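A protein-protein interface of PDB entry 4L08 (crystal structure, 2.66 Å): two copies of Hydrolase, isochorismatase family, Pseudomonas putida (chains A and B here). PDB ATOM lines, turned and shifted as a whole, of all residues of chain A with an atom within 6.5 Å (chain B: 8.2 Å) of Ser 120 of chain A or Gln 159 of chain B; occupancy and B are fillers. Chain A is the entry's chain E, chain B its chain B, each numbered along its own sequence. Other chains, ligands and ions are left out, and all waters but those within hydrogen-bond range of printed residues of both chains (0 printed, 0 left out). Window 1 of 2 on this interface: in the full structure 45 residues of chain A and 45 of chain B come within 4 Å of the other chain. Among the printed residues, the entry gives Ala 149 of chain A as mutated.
N of Ser 120 of chain A sits close to NE2 of Gln 159 of chain B.
The side-chain amide nitrogen of Gln 159 of chain B lies close to the backbone NH of Ala 119 of chain A (3.0 Å).
The side-chain hydroxyl (OG) of Ser 120 of chain A sits at hydrogen-bond distance from the side-chain carboxylate (OD2) of Asp 156 of chain A, 2.6 Å away.
The backbone carbonyl oxygen of Ala 119 of chain A lies within hydrogen-bond range of the side-chain amino group of Lys 116 of chain A, 2.9 Å away.
OD1 of Asp 156 of chain B sits close to OE1 of Gln 159 of chain B, at 3.0 Å.
O of Asp 156 of chain B is in hydrogen-bond range of OG of Ser 160 of chain B (2.7 Å).
O of Val 155 of chain B lies close to OE1 of Gln 159 of chain B (3.4 Å).
The side-chain hydroxyl of Ser 120 of chain A lies within hydrogen-bond range of the backbone NH of Phe 122 of chain A, at 3.1 Å.
Pro 81 of chain A touches Val 158 of chain B (CG to O, 3.6 Å).
Pro 81 of chain A touches Gly 161 of chain B (CG to C, 3.5 Å).
Pro 81 of chain A touches Phe 162 of chain B.
Pro 81 of chain A touches Lys 163 of chain B.
CA of Trp 82 of chain A touches CG1 of Val 158 of chain B, 3.8 Å away.
Trp 82 of chain A touches Tyr 190 of chain B (NE1 to CD1, 3.7 Å).
NE2 of Gln 159 of chain B touches C of Gly 118 of chain A, 3.7 Å away.
O of Gln 159 of chain B touches CE2 of Phe 123 of chain A, 3.3 Å away.
Ser 160 of chain B touches Phe 123 of chain A.
OD1 of Asp 156 of chain A touches CD1 of Phe 123 of chain B, at 3.9 Å.
Printed residues of chain B within 4 Å of Pro 81 of chain A: Val 158, Gly 161, Phe 162 and Lys 163.
Of the printed residues of chain B, Trp 82 of chain A touches Val 158 and Tyr 190.
Of chain B, only Gln 159 (2.8 Å) comes within 4 Å of Ser 120 of chain A.
No residue of chain B comes within 4 Å of Ser 121 of chain A.
Of the printed residues of chain B, Phe 123 of chain A touches Gln 159 and Ser 160.
Thr 153 of chain A touches none of the printed residues of chain B.
Of the printed residues of chain B, Asp 156 of chain A touches Phe 123.
Ser 120 of chain B touches none of the printed residues of chain A.
Gln 159 of chain B touches just these residues of chain A: Gly 118, Ala 119, Ser 120 and Phe 123.
Of the printed residues of chain A, Tyr 190 of chain B touches Trp 82 and Gly 148.
The nearest residue of chain B that does not touch Ser 120 of chain A is Asp 156 of chain B (5.4 Å).
The nearest printed residue of chain B that does not touch Phe 123 of chain A is Asp 156 of chain B (4.3 Å).
Hydrophobic or aromatic side chains of chain B that line the printed part of chain A: Phe 123, Val 158 and Tyr 190.
Among the printed residues, 13 pairs touch across the chains.
Among the printed residues, no Asp or Glu carboxylate lies within 4 Å of a Lys or Arg side-chain nitrogen of the other chain.
Asp 156 of chain A touches Phe 123 of chain B, but with the chains exchanged Phe 123 of chain A does not touch Asp 156 of chain B (4.3 Å).
Of the 13 pairs that touch across the chains among the printed residues, none has its exchanged pair printed and touching as well.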
ATOM      1  N   LEU A  80     -25.030  -2.336  21.711  1.00  0.00           N
ATOM      2  CA  LEU A  80     -25.482  -1.696  20.470  1.00  0.00           C
ATOM      3  C   LEU A  80     -27.005  -1.627  20.318  1.00  0.00           C
ATOM      4  O   LEU A  80     -27.660  -2.658  20.136  1.00  0.00           O
ATOM      5  CB  LEU A  80     -24.854  -2.378  19.247  1.00  0.00           C
ATOM      6  CG  LEU A  80     -23.358  -2.160  18.990  1.00  0.00           C
ATOM      7  CD1 LEU A  80     -22.830  -3.214  18.034  1.00  0.00           C
ATOM      8  CD2 LEU A  80     -23.062  -0.763  18.459  1.00  0.00           C
ATOM      9  N   PRO A  81     -27.570  -0.403  20.372  1.00  0.00           N
ATOM     10  CA  PRO A  81     -29.024  -0.177  20.326  1.00  0.00           C
ATOM     11  C   PRO A  81     -29.711  -0.648  19.042  1.00  0.00           C
ATOM     12  O   PRO A  81     -30.933  -0.804  19.029  1.00  0.00           O
ATOM     13  CB  PRO A  81     -29.154   1.348  20.463  1.00  0.00           C
ATOM     14  CG  PRO A  81     -27.827   1.891  20.061  1.00  0.00           C
ATOM     15  CD  PRO A  81     -26.828   0.865  20.505  1.00  0.00           C
ATOM     16  N   TRP A  82     -28.933  -0.866  17.982  1.00  0.00           N
ATOM     17  CA  TRP A  82     -29.463  -1.350  16.704  1.00  0.00           C
ATOM     18  C   TRP A  82     -29.898  -2.783  16.791  1.00  0.00           C
ATOM     19  O   TRP A  82     -30.878  -3.187  16.158  1.00  0.00           O
ATOM     20  CB  TRP A  82     -28.430  -1.183  15.595  1.00  0.00           C
ATOM     21  CG  TRP A  82     -28.970  -1.439  14.205  1.00  0.00           C
ATOM     22  CD1 TRP A  82     -30.173  -0.992  13.664  1.00  0.00           C
ATOM     23  CD2 TRP A  82     -28.325  -2.193  13.118  1.00  0.00           C
ATOM     24  NE1 TRP A  82     -30.317  -1.415  12.368  1.00  0.00           N
ATOM     25  CE2 TRP A  82     -29.247  -2.137  11.977  1.00  0.00           C
ATOM     26  CE3 TRP A  82     -27.124  -2.886  12.981  1.00  0.00           C
ATOM     27  CZ2 TRP A  82     -28.959  -2.754  10.767  1.00  0.00           C
ATOM     28  CZ3 TRP A  82     -26.844  -3.502  11.756  1.00  0.00           C
ATOM     29  CH2 TRP A  82     -27.741  -3.436  10.676  1.00  0.00           C
ATOM     30  N   LYS A 116     -17.996  -4.546   9.589  1.00  0.00           N
ATOM     31  CA  LYS A 116     -18.734  -3.396  10.100  1.00  0.00           C
ATOM     32  C   LYS A 116     -19.774  -3.842  11.123  1.00  0.00           C
ATOM     33  O   LYS A 116     -20.114  -5.024  11.191  1.00  0.00           O
ATOM     34  CB  LYS A 116     -19.400  -2.637   8.949  1.00  0.00           C
ATOM     35  CG  LYS A 116     -20.450  -3.432   8.185  1.00  0.00           C
ATOM     36  CD  LYS A 116     -20.686  -2.824   6.816  1.00  0.00           C
ATOM     37  CE  LYS A 116     -21.743  -3.582   6.033  1.00  0.00           C
ATOM     38  NZ  LYS A 116     -23.127  -3.321   6.522  1.00  0.00           N
ATOM     39  N   LYS A 117     -20.279  -2.894  11.908  1.00  0.00           N
ATOM     40  CA  LYS A 117     -21.230  -3.198  12.979  1.00  0.00           C
ATOM     41  C   LYS A 117     -22.603  -2.559  12.755  1.00  0.00           C
ATOM     42  O   LYS A 117     -23.520  -2.745  13.559  1.00  0.00           O
ATOM     43  CB  LYS A 117     -20.663  -2.775  14.344  1.00  0.00           C
ATOM     44  CG  LYS A 117     -19.212  -3.170  14.595  1.00  0.00           C
ATOM     45  CD  LYS A 117     -19.038  -4.645  14.925  1.00  0.00           C
ATOM     46  CE  LYS A 117     -17.563  -5.011  14.970  1.00  0.00           C
ATOM     47  NZ  LYS A 117     -17.340  -6.457  15.245  1.00  0.00           N
ATOM     48  N   GLY A 118     -22.739  -1.809  11.664  1.00  0.00           N
ATOM     49  CA  GLY A 118     -23.996  -1.144  11.330  1.00  0.00           C
ATOM     50  C   GLY A 118     -24.479  -1.441   9.923  1.00  0.00           C
ATOM     51  O   GLY A 118     -23.978  -2.352   9.262  1.00  0.00           O
ATOM     52  N   ALA A 119     -25.464  -0.667   9.475  1.00  0.00           N
ATOM     53  CA  ALA A 119     -26.006  -0.780   8.122  1.00  0.00           C
ATOM     54  C   ALA A 119     -25.028  -0.240   7.077  1.00  0.00           C
ATOM     55  O   ALA A 119     -24.701  -0.935   6.116  1.00  0.00           O
ATOM     56  CB  ALA A 119     -27.349  -0.068   8.022  1.00  0.00           C
ATOM     57  N   SER A 120     -24.557   0.989   7.274  1.00  0.00           N
ATOM     58  CA  SER A 120     -23.630   1.619   6.336  1.00  0.00           C
ATOM     59  C   SER A 120     -22.251   0.970   6.361  1.00  0.00           C
ATOM     60  O   SER A 120     -21.731   0.624   7.422  1.00  0.00           O
ATOM     61  CB  SER A 120     -23.500   3.115   6.614  1.00  0.00           C
ATOM     62  OG  SER A 120     -22.513   3.694   5.773  1.00  0.00           O
ATOM     63  N   SER A 121     -21.669   0.820   5.178  1.00  0.00           N
ATOM     64  CA  SER A 121     -20.338   0.246   5.037  1.00  0.00           C
ATOM     65  C   SER A 121     -19.237   1.241   5.401  1.00  0.00           C
ATOM     66  O   SER A 121     -18.077   0.859   5.561  1.00  0.00           O
ATOM     67  CB  SER A 121     -20.137  -0.281   3.616  1.00  0.00           C
ATOM     68  OG  SER A 121     -20.969  -1.399   3.364  1.00  0.00           O
ATOM     69  N   PHE A 122     -19.610   2.514   5.530  1.00  0.00           N
ATOM     70  CA  PHE A 122     -18.658   3.586   5.826  1.00  0.00           C
ATOM     71  C   PHE A 122     -18.583   3.896   7.316  1.00  0.00           C
ATOM     72  O   PHE A 122     -17.523   4.276   7.816  1.00  0.00           O
ATOM     73  CB  PHE A 122     -19.016   4.865   5.061  1.00  0.00           C
ATOM     74  CG  PHE A 122     -18.699   4.812   3.591  1.00  0.00           C
ATOM     75  CD1 PHE A 122     -19.574   4.206   2.693  1.00  0.00           C
ATOM     76  CD2 PHE A 122     -17.530   5.384   3.100  1.00  0.00           C
ATOM     77  CE1 PHE A 122     -19.283   4.160   1.340  1.00  0.00           C
ATOM     78  CE2 PHE A 122     -17.232   5.343   1.746  1.00  0.00           C
ATOM     79  CZ  PHE A 122     -18.111   4.730   0.866  1.00  0.00           C
ATOM     80  N   PHE A 123     -19.702   3.738   8.023  1.00  0.00           N
ATOM     81  CA  PHE A 123     -19.744   4.095   9.437  1.00  0.00           C
ATOM     82  C   PHE A 123     -18.915   3.151  10.299  1.00  0.00           C
ATOM     83  O   PHE A 123     -19.096   1.932  10.252  1.00  0.00           O
ATOM     84  CB  PHE A 123     -21.180   4.189   9.975  1.00  0.00           C
ATOM     85  CG  PHE A 123     -21.257   4.786  11.355  1.00  0.00           C
ATOM     86  CD1 PHE A 123     -21.299   6.170  11.527  1.00  0.00           C
ATOM     87  CD2 PHE A 123     -21.243   3.971  12.487  1.00  0.00           C
ATOM     88  CE1 PHE A 123     -21.346   6.727  12.797  1.00  0.00           C
ATOM     89  CE2 PHE A 123     -21.288   4.524  13.759  1.00  0.00           C
ATOM     90  CZ  PHE A 123     -21.341   5.903  13.913  1.00  0.00           C
ATOM     91  N   GLY A 124     -18.008   3.733  11.081  1.00  0.00           N
ATOM     92  CA  GLY A 124     -17.146   2.974  11.981  1.00  0.00           C
ATOM     93  C   GLY A 124     -16.302   1.915  11.293  1.00  0.00           C
ATOM     94  O   GLY A 124     -16.027   0.860  11.867  1.00  0.00           O
ATOM     95  N   SER A 125     -15.900   2.201  10.056  1.00  0.00           N
ATOM     96  CA  SER A 125     -15.069   1.292   9.273  1.00  0.00           C
ATOM     97  C   SER A 125     -13.985   2.069   8.531  1.00  0.00           C
ATOM     98  O   SER A 125     -14.000   3.298   8.502  1.00  0.00           O
ATOM     99  CB  SER A 125     -15.922   0.479   8.289  1.00  0.00           C
ATOM    100  OG  SER A 125     -16.062   1.148   7.047  1.00  0.00           O
ATOM    101  N   GLY A 148     -31.785  -1.429   3.023  1.00  0.00           N
ATOM    102  CA  GLY A 148     -31.024  -1.464   4.263  1.00  0.00           C
ATOM    103  C   GLY A 148     -29.614  -0.941   4.085  1.00  0.00           C
ATOM    104  O   GLY A 148     -29.401   0.269   3.974  1.00  0.00           O
ATOM    105  N   ALA A 149     -28.655  -1.863   4.044  1.00  0.00           N
ATOM    106  CA  ALA A 149     -27.234  -1.524   3.996  1.00  0.00           C
ATOM    107  C   ALA A 149     -26.788  -0.900   2.673  1.00  0.00           C
ATOM    108  O   ALA A 149     -25.849  -0.106   2.652  1.00  0.00           O
ATOM    109  CB  ALA A 149     -26.391  -2.749   4.309  1.00  0.00           C
ATOM    110  N   ALA A 152     -27.948   2.878   2.767  1.00  0.00           N
ATOM    111  CA  ALA A 152     -27.110   3.541   3.764  1.00  0.00           C
ATOM    112  C   ALA A 152     -25.676   3.753   3.271  1.00  0.00           C
ATOM    113  O   ALA A 152     -25.065   4.788   3.554  1.00  0.00           O
ATOM    114  CB  ALA A 152     -27.118   2.758   5.070  1.00  0.00           C
ATOM    115  N   THR A 153     -25.155   2.771   2.536  1.00  0.00           N
ATOM    116  CA  THR A 153     -23.803   2.834   1.980  1.00  0.00           C
ATOM    117  C   THR A 153     -23.742   3.845   0.839  1.00  0.00           C
ATOM    118  O   THR A 153     -22.779   4.603   0.734  1.00  0.00           O
ATOM    119  CB  THR A 153     -23.316   1.444   1.511  1.00  0.00           C
ATOM    120  OG1 THR A 153     -23.308   0.542   2.626  1.00  0.00           O
ATOM    121  CG2 THR A 153     -21.907   1.517   0.919  1.00  0.00           C
ATOM    122  N   VAL A 154     -24.782   3.853   0.004  1.00  0.00           N
ATOM    123  CA  VAL A 154     -24.905   4.804  -1.100  1.00  0.00           C
ATOM    124  C   VAL A 154     -24.875   6.239  -0.582  1.00  0.00           C
ATOM    125  O   VAL A 154     -24.067   7.043  -1.049  1.00  0.00           O
ATOM    126  CB  VAL A 154     -26.187   4.558  -1.935  1.00  0.00           C
ATOM    127  CG1 VAL A 154     -26.478   5.735  -2.857  1.00  0.00           C
ATOM    128  CG2 VAL A 154     -26.055   3.279  -2.749  1.00  0.00           C
ATOM    129  N   ASP A 156     -23.848   7.396   2.333  1.00  0.00           N
ATOM    130  CA  ASP A 156     -22.547   7.669   2.934  1.00  0.00           C
ATOM    131  C   ASP A 156     -21.459   7.895   1.889  1.00  0.00           C
ATOM    132  O   ASP A 156     -20.585   8.743   2.076  1.00  0.00           O
ATOM    133  CB  ASP A 156     -22.147   6.545   3.893  1.00  0.00           C
ATOM    134  CG  ASP A 156     -22.410   6.892   5.354  1.00  0.00           C
ATOM    135  OD1 ASP A 156     -23.134   7.881   5.632  1.00  0.00           O
ATOM    136  OD2 ASP A 156     -21.881   6.172   6.230  1.00  0.00           O
ATOM    137  N   ALA A 157     -21.530   7.143   0.792  1.00  0.00           N
ATOM    138  CA  ALA A 157     -20.561   7.252  -0.299  1.00  0.00           C
ATOM    139  C   ALA A 157     -20.544   8.647  -0.926  1.00  0.00           C
ATOM    140  O   ALA A 157     -19.471   9.215  -1.144  1.00  0.00           O
ATOM    141  CB  ALA A 157     -20.814   6.184  -1.355  1.00  0.00           C
ATOM    142  N   SER B 120     -27.281  13.413   6.264  1.00  0.00           N
ATOM    143  CA  SER B 120     -27.247  13.024   7.673  1.00  0.00           C
ATOM    144  C   SER B 120     -26.706  14.133   8.574  1.00  0.00           C
ATOM    145  O   SER B 120     -25.773  14.852   8.208  1.00  0.00           O
ATOM    146  CB  SER B 120     -26.414  11.757   7.857  1.00  0.00           C
ATOM    147  OG  SER B 120     -26.257  11.449   9.231  1.00  0.00           O
ATOM    148  N   PHE B 122     -25.227  13.652  11.412  1.00  0.00           N
ATOM    149  CA  PHE B 122     -24.045  13.164  12.123  1.00  0.00           C
ATOM    150  C   PHE B 122     -22.777  13.205  11.272  1.00  0.00           C
ATOM    151  O   PHE B 122     -21.676  13.335  11.806  1.00  0.00           O
ATOM    152  CB  PHE B 122     -24.277  11.743  12.640  1.00  0.00           C
ATOM    153  CG  PHE B 122     -25.216  11.665  13.811  1.00  0.00           C
ATOM    154  CD1 PHE B 122     -26.596  11.711  13.622  1.00  0.00           C
ATOM    155  CD2 PHE B 122     -24.721  11.537  15.104  1.00  0.00           C
ATOM    156  CE1 PHE B 122     -27.460  11.642  14.700  1.00  0.00           C
ATOM    157  CE2 PHE B 122     -25.582  11.463  16.187  1.00  0.00           C
ATOM    158  CZ  PHE B 122     -26.953  11.515  15.984  1.00  0.00           C
ATOM    159  N   PHE B 123     -22.938  13.098   9.955  1.00  0.00           N
ATOM    160  CA  PHE B 123     -21.800  13.020   9.043  1.00  0.00           C
ATOM    161  C   PHE B 123     -21.065  14.350   8.918  1.00  0.00           C
ATOM    162  O   PHE B 123     -21.653  15.365   8.546  1.00  0.00           O
ATOM    163  CB  PHE B 123     -22.229  12.521   7.657  1.00  0.00           C
ATOM    164  CG  PHE B 123     -21.074  12.118   6.783  1.00  0.00           C
ATOM    165  CD1 PHE B 123     -20.730  10.778   6.641  1.00  0.00           C
ATOM    166  CD2 PHE B 123     -20.309  13.081   6.122  1.00  0.00           C
ATOM    167  CE1 PHE B 123     -19.654  10.404   5.846  1.00  0.00           C
ATOM    168  CE2 PHE B 123     -19.229  12.713   5.334  1.00  0.00           C
ATOM    169  CZ  PHE B 123     -18.902  11.374   5.195  1.00  0.00           C
ATOM    170  N   SER B 128     -22.573  14.133  17.162  1.00  0.00           N
ATOM    171  CA  SER B 128     -22.230  12.969  17.975  1.00  0.00           C
ATOM    172  C   SER B 128     -21.521  13.336  19.289  1.00  0.00           C
ATOM    173  O   SER B 128     -21.870  12.818  20.354  1.00  0.00           O
ATOM    174  CB  SER B 128     -21.376  11.999  17.166  1.00  0.00           C
ATOM    175  OG  SER B 128     -21.001  10.894  17.958  1.00  0.00           O
ATOM    176  N   ARG B 151     -34.343  10.417   7.820  1.00  0.00           N
ATOM    177  CA  ARG B 151     -33.932   9.009   7.766  1.00  0.00           C
ATOM    178  C   ARG B 151     -32.415   8.844   7.893  1.00  0.00           C
ATOM    179  O   ARG B 151     -31.941   8.011   8.670  1.00  0.00           O
ATOM    180  CB  ARG B 151     -34.423   8.326   6.488  1.00  0.00           C
ATOM    181  CG  ARG B 151     -34.205   6.821   6.520  1.00  0.00           C
ATOM    182  CD  ARG B 151     -33.774   6.280   5.172  1.00  0.00           C
ATOM    183  NE  ARG B 151     -34.882   5.681   4.435  1.00  0.00           N
ATOM    184  CZ  ARG B 151     -35.011   4.378   4.197  1.00  0.00           C
ATOM    185  NH1 ARG B 151     -34.095   3.513   4.631  1.00  0.00           N
ATOM    186  NH2 ARG B 151     -36.060   3.941   3.510  1.00  0.00           N
ATOM    187  N   ALA B 152     -31.667   9.640   7.130  1.00  0.00           N
ATOM    188  CA  ALA B 152     -30.204   9.640   7.195  1.00  0.00           C
ATOM    189  C   ALA B 152     -29.687   9.946   8.604  1.00  0.00           C
ATOM    190  O   ALA B 152     -28.718   9.337   9.059  1.00  0.00           O
ATOM    191  CB  ALA B 152     -29.627  10.619   6.183  1.00  0.00           C
ATOM    192  N   THR B 153     -30.346  10.879   9.291  1.00  0.00           N
ATOM    193  CA  THR B 153     -30.032  11.192  10.687  1.00  0.00           C
ATOM    194  C   THR B 153     -30.428  10.040  11.617  1.00  0.00           C
ATOM    195  O   THR B 153     -29.662   9.671  12.513  1.00  0.00           O
ATOM    196  CB  THR B 153     -30.714  12.502  11.132  1.00  0.00           C
ATOM    197  OG1 THR B 153     -30.279  13.574  10.285  1.00  0.00           O
ATOM    198  CG2 THR B 153     -30.391  12.835  12.587  1.00  0.00           C
ATOM    199  N   VAL B 154     -31.617   9.476  11.392  1.00  0.00           N
ATOM    200  CA  VAL B 154     -32.120   8.347  12.174  1.00  0.00           C
ATOM    201  C   VAL B 154     -31.145   7.169  12.104  1.00  0.00           C
ATOM    202  O   VAL B 154     -30.725   6.655  13.139  1.00  0.00           O
ATOM    203  CB  VAL B 154     -33.544   7.925  11.724  1.00  0.00           C
ATOM    204  CG1 VAL B 154     -33.933   6.562  12.285  1.00  0.00           C
ATOM    205  CG2 VAL B 154     -34.566   8.974  12.133  1.00  0.00           C
ATOM    206  N   VAL B 155     -30.774   6.774  10.884  1.00  0.00           N
ATOM    207  CA  VAL B 155     -29.832   5.671  10.656  1.00  0.00           C
ATOM    208  C   VAL B 155     -28.486   5.922  11.343  1.00  0.00           C
ATOM    209  O   VAL B 155     -27.960   5.043  12.029  1.00  0.00           O
ATOM    210  CB  VAL B 155     -29.636   5.389   9.142  1.00  0.00           C
ATOM    211  CG1 VAL B 155     -28.446   4.467   8.896  1.00  0.00           C
ATOM    212  CG2 VAL B 155     -30.901   4.788   8.541  1.00  0.00           C
ATOM    213  N   ASP B 156     -27.944   7.124  11.167  1.00  0.00           N
ATOM    214  CA  ASP B 156     -26.675   7.487  11.793  1.00  0.00           C
ATOM    215  C   ASP B 156     -26.754   7.589  13.314  1.00  0.00           C
ATOM    216  O   ASP B 156     -25.760   7.347  14.001  1.00  0.00           O
ATOM    217  CB  ASP B 156     -26.118   8.783  11.196  1.00  0.00           C
ATOM    218  CG  ASP B 156     -25.114   8.531  10.074  1.00  0.00           C
ATOM    219  OD1 ASP B 156     -24.969   7.366   9.632  1.00  0.00           O
ATOM    220  OD2 ASP B 156     -24.460   9.504   9.633  1.00  0.00           O
ATOM    221  N   ALA B 157     -27.929   7.940  13.835  1.00  0.00           N
ATOM    222  CA  ALA B 157     -28.126   8.050  15.282  1.00  0.00           C
ATOM    223  C   ALA B 157     -28.101   6.692  15.990  1.00  0.00           C
ATOM    224  O   ALA B 157     -27.482   6.559  17.048  1.00  0.00           O
ATOM    225  CB  ALA B 157     -29.408   8.807  15.599  1.00  0.00           C
ATOM    226  N   VAL B 158     -28.764   5.693  15.405  1.00  0.00           N
ATOM    227  CA  VAL B 158     -28.765   4.334  15.965  1.00  0.00           C
ATOM    228  C   VAL B 158     -27.373   3.728  15.880  1.00  0.00           C
ATOM    229  O   VAL B 158     -26.920   3.066  16.814  1.00  0.00           O
ATOM    230  CB  VAL B 158     -29.722   3.367  15.230  1.00  0.00           C
ATOM    231  CG1 VAL B 158     -30.274   2.339  16.204  1.00  0.00           C
ATOM    232  CG2 VAL B 158     -30.857   4.112  14.553  1.00  0.00           C
ATOM    233  N   GLN B 159     -26.710   3.950  14.748  1.00  0.00           N
ATOM    234  CA  GLN B 159     -25.357   3.457  14.532  1.00  0.00           C
ATOM    235  C   GLN B 159     -24.374   4.066  15.525  1.00  0.00           C
ATOM    236  O   GLN B 159     -23.430   3.402  15.943  1.00  0.00           O
ATOM    237  CB  GLN B 159     -24.903   3.745  13.102  1.00  0.00           C
ATOM    238  CG  GLN B 159     -25.533   2.839  12.055  1.00  0.00           C
ATOM    239  CD  GLN B 159     -25.164   3.229  10.638  1.00  0.00           C
ATOM    240  OE1 GLN B 159     -25.048   4.413  10.307  1.00  0.00           O
ATOM    241  NE2 GLN B 159     -24.983   2.234   9.788  1.00  0.00           N
ATOM    242  N   SER B 160     -24.622   5.318  15.907  1.00  0.00           N
ATOM    243  CA  SER B 160     -23.748   6.073  16.809  1.00  0.00           C
ATOM    244  C   SER B 160     -23.882   5.691  18.287  1.00  0.00           C
ATOM    245  O   SER B 160     -23.116   6.175  19.121  1.00  0.00           O
ATOM    246  CB  SER B 160     -23.985   7.576  16.643  1.00  0.00           C
ATOM    247  OG  SER B 160     -23.582   8.014  15.359  1.00  0.00           O
ATOM    248  N   GLY B 161     -24.850   4.836  18.604  1.00  0.00           N
ATOM    249  CA  GLY B 161     -25.034   4.343  19.968  1.00  0.00           C
ATOM    250  C   GLY B 161     -26.199   4.953  20.728  1.00  0.00           C
ATOM    251  O   GLY B 161     -26.277   4.830  21.953  1.00  0.00           O
ATOM    252  N   PHE B 162     -27.115   5.594  20.007  1.00  0.00           N
ATOM    253  CA  PHE B 162     -28.264   6.247  20.625  1.00  0.00           C
ATOM    254  C   PHE B 162     -29.578   5.609  20.199  1.00  0.00           C
ATOM    255  O   PHE B 162     -29.737   5.207  19.049  1.00  0.00           O
ATOM    256  CB  PHE B 162     -28.276   7.735  20.281  1.00  0.00           C
ATOM    257  CG  PHE B 162     -26.965   8.423  20.536  1.00  0.00           C
ATOM    258  CD1 PHE B 162     -26.595   8.784  21.827  1.00  0.00           C
ATOM    259  CD2 PHE B 162     -26.100   8.707  19.486  1.00  0.00           C
ATOM    260  CE1 PHE B 162     -25.386   9.413  22.065  1.00  0.00           C
ATOM    261  CE2 PHE B 162     -24.888   9.335  19.719  1.00  0.00           C
ATOM    262  CZ  PHE B 162     -24.529   9.688  21.010  1.00  0.00           C
ATOM    263  N   LYS B 163     -30.515   5.523  21.137  1.00  0.00           N
ATOM    264  CA  LYS B 163     -31.853   5.016  20.856  1.00  0.00           C
ATOM    265  C   LYS B 163     -32.697   6.108  20.196  1.00  0.00           C
ATOM    266  O   LYS B 163     -32.678   7.263  20.626  1.00  0.00           O
ATOM    267  CB  LYS B 163     -32.508   4.512  22.141  1.00  0.00           C
ATOM    268  CG  LYS B 163     -31.852   3.262  22.707  1.00  0.00           C
ATOM    269  CD  LYS B 163     -32.088   3.132  24.204  1.00  0.00           C
ATOM    270  CE  LYS B 163     -31.385   1.908  24.779  1.00  0.00           C
ATOM    271  NZ  LYS B 163     -31.906   0.622  24.232  1.00  0.00           N
ATOM    272  N   VAL B 164     -33.430   5.739  19.149  1.00  0.00           N
ATOM    273  CA  VAL B 164     -34.115   6.722  18.311  1.00  0.00           C
ATOM    274  C   VAL B 164     -35.637   6.629  18.395  1.00  0.00           C
ATOM    275  O   VAL B 164     -36.228   5.562  18.204  1.00  0.00           O
ATOM    276  CB  VAL B 164     -33.658   6.621  16.837  1.00  0.00           C
ATOM    277  CG1 VAL B 164     -34.413   7.606  15.952  1.00  0.00           C
ATOM    278  CG2 VAL B 164     -32.160   6.858  16.734  1.00  0.00           C
ATOM    279  N   TYR B 190     -34.684   0.796  12.541  1.00  0.00           N
ATOM    280  CA  TYR B 190     -33.847   1.837  13.152  1.00  0.00           C
ATOM    281  C   TYR B 190     -34.373   2.489  14.433  1.00  0.00           C
ATOM    282  O   TYR B 190     -33.590   2.795  15.332  1.00  0.00           O
ATOM    283  CB  TYR B 190     -33.483   2.904  12.113  1.00  0.00           C
ATOM    284  CG  TYR B 190     -32.932   2.330  10.825  1.00  0.00           C
ATOM    285  CD1 TYR B 190     -31.697   1.685  10.799  1.00  0.00           C
ATOM    286  CD2 TYR B 190     -33.652   2.425   9.634  1.00  0.00           C
ATOM    287  CE1 TYR B 190     -31.192   1.150   9.625  1.00  0.00           C
ATOM    288  CE2 TYR B 190     -33.155   1.896   8.451  1.00  0.00           C
ATOM    289  CZ  TYR B 190     -31.924   1.259   8.454  1.00  0.00           C
ATOM    290  OH  TYR B 190     -31.423   0.732   7.287  1.00  0.00           O
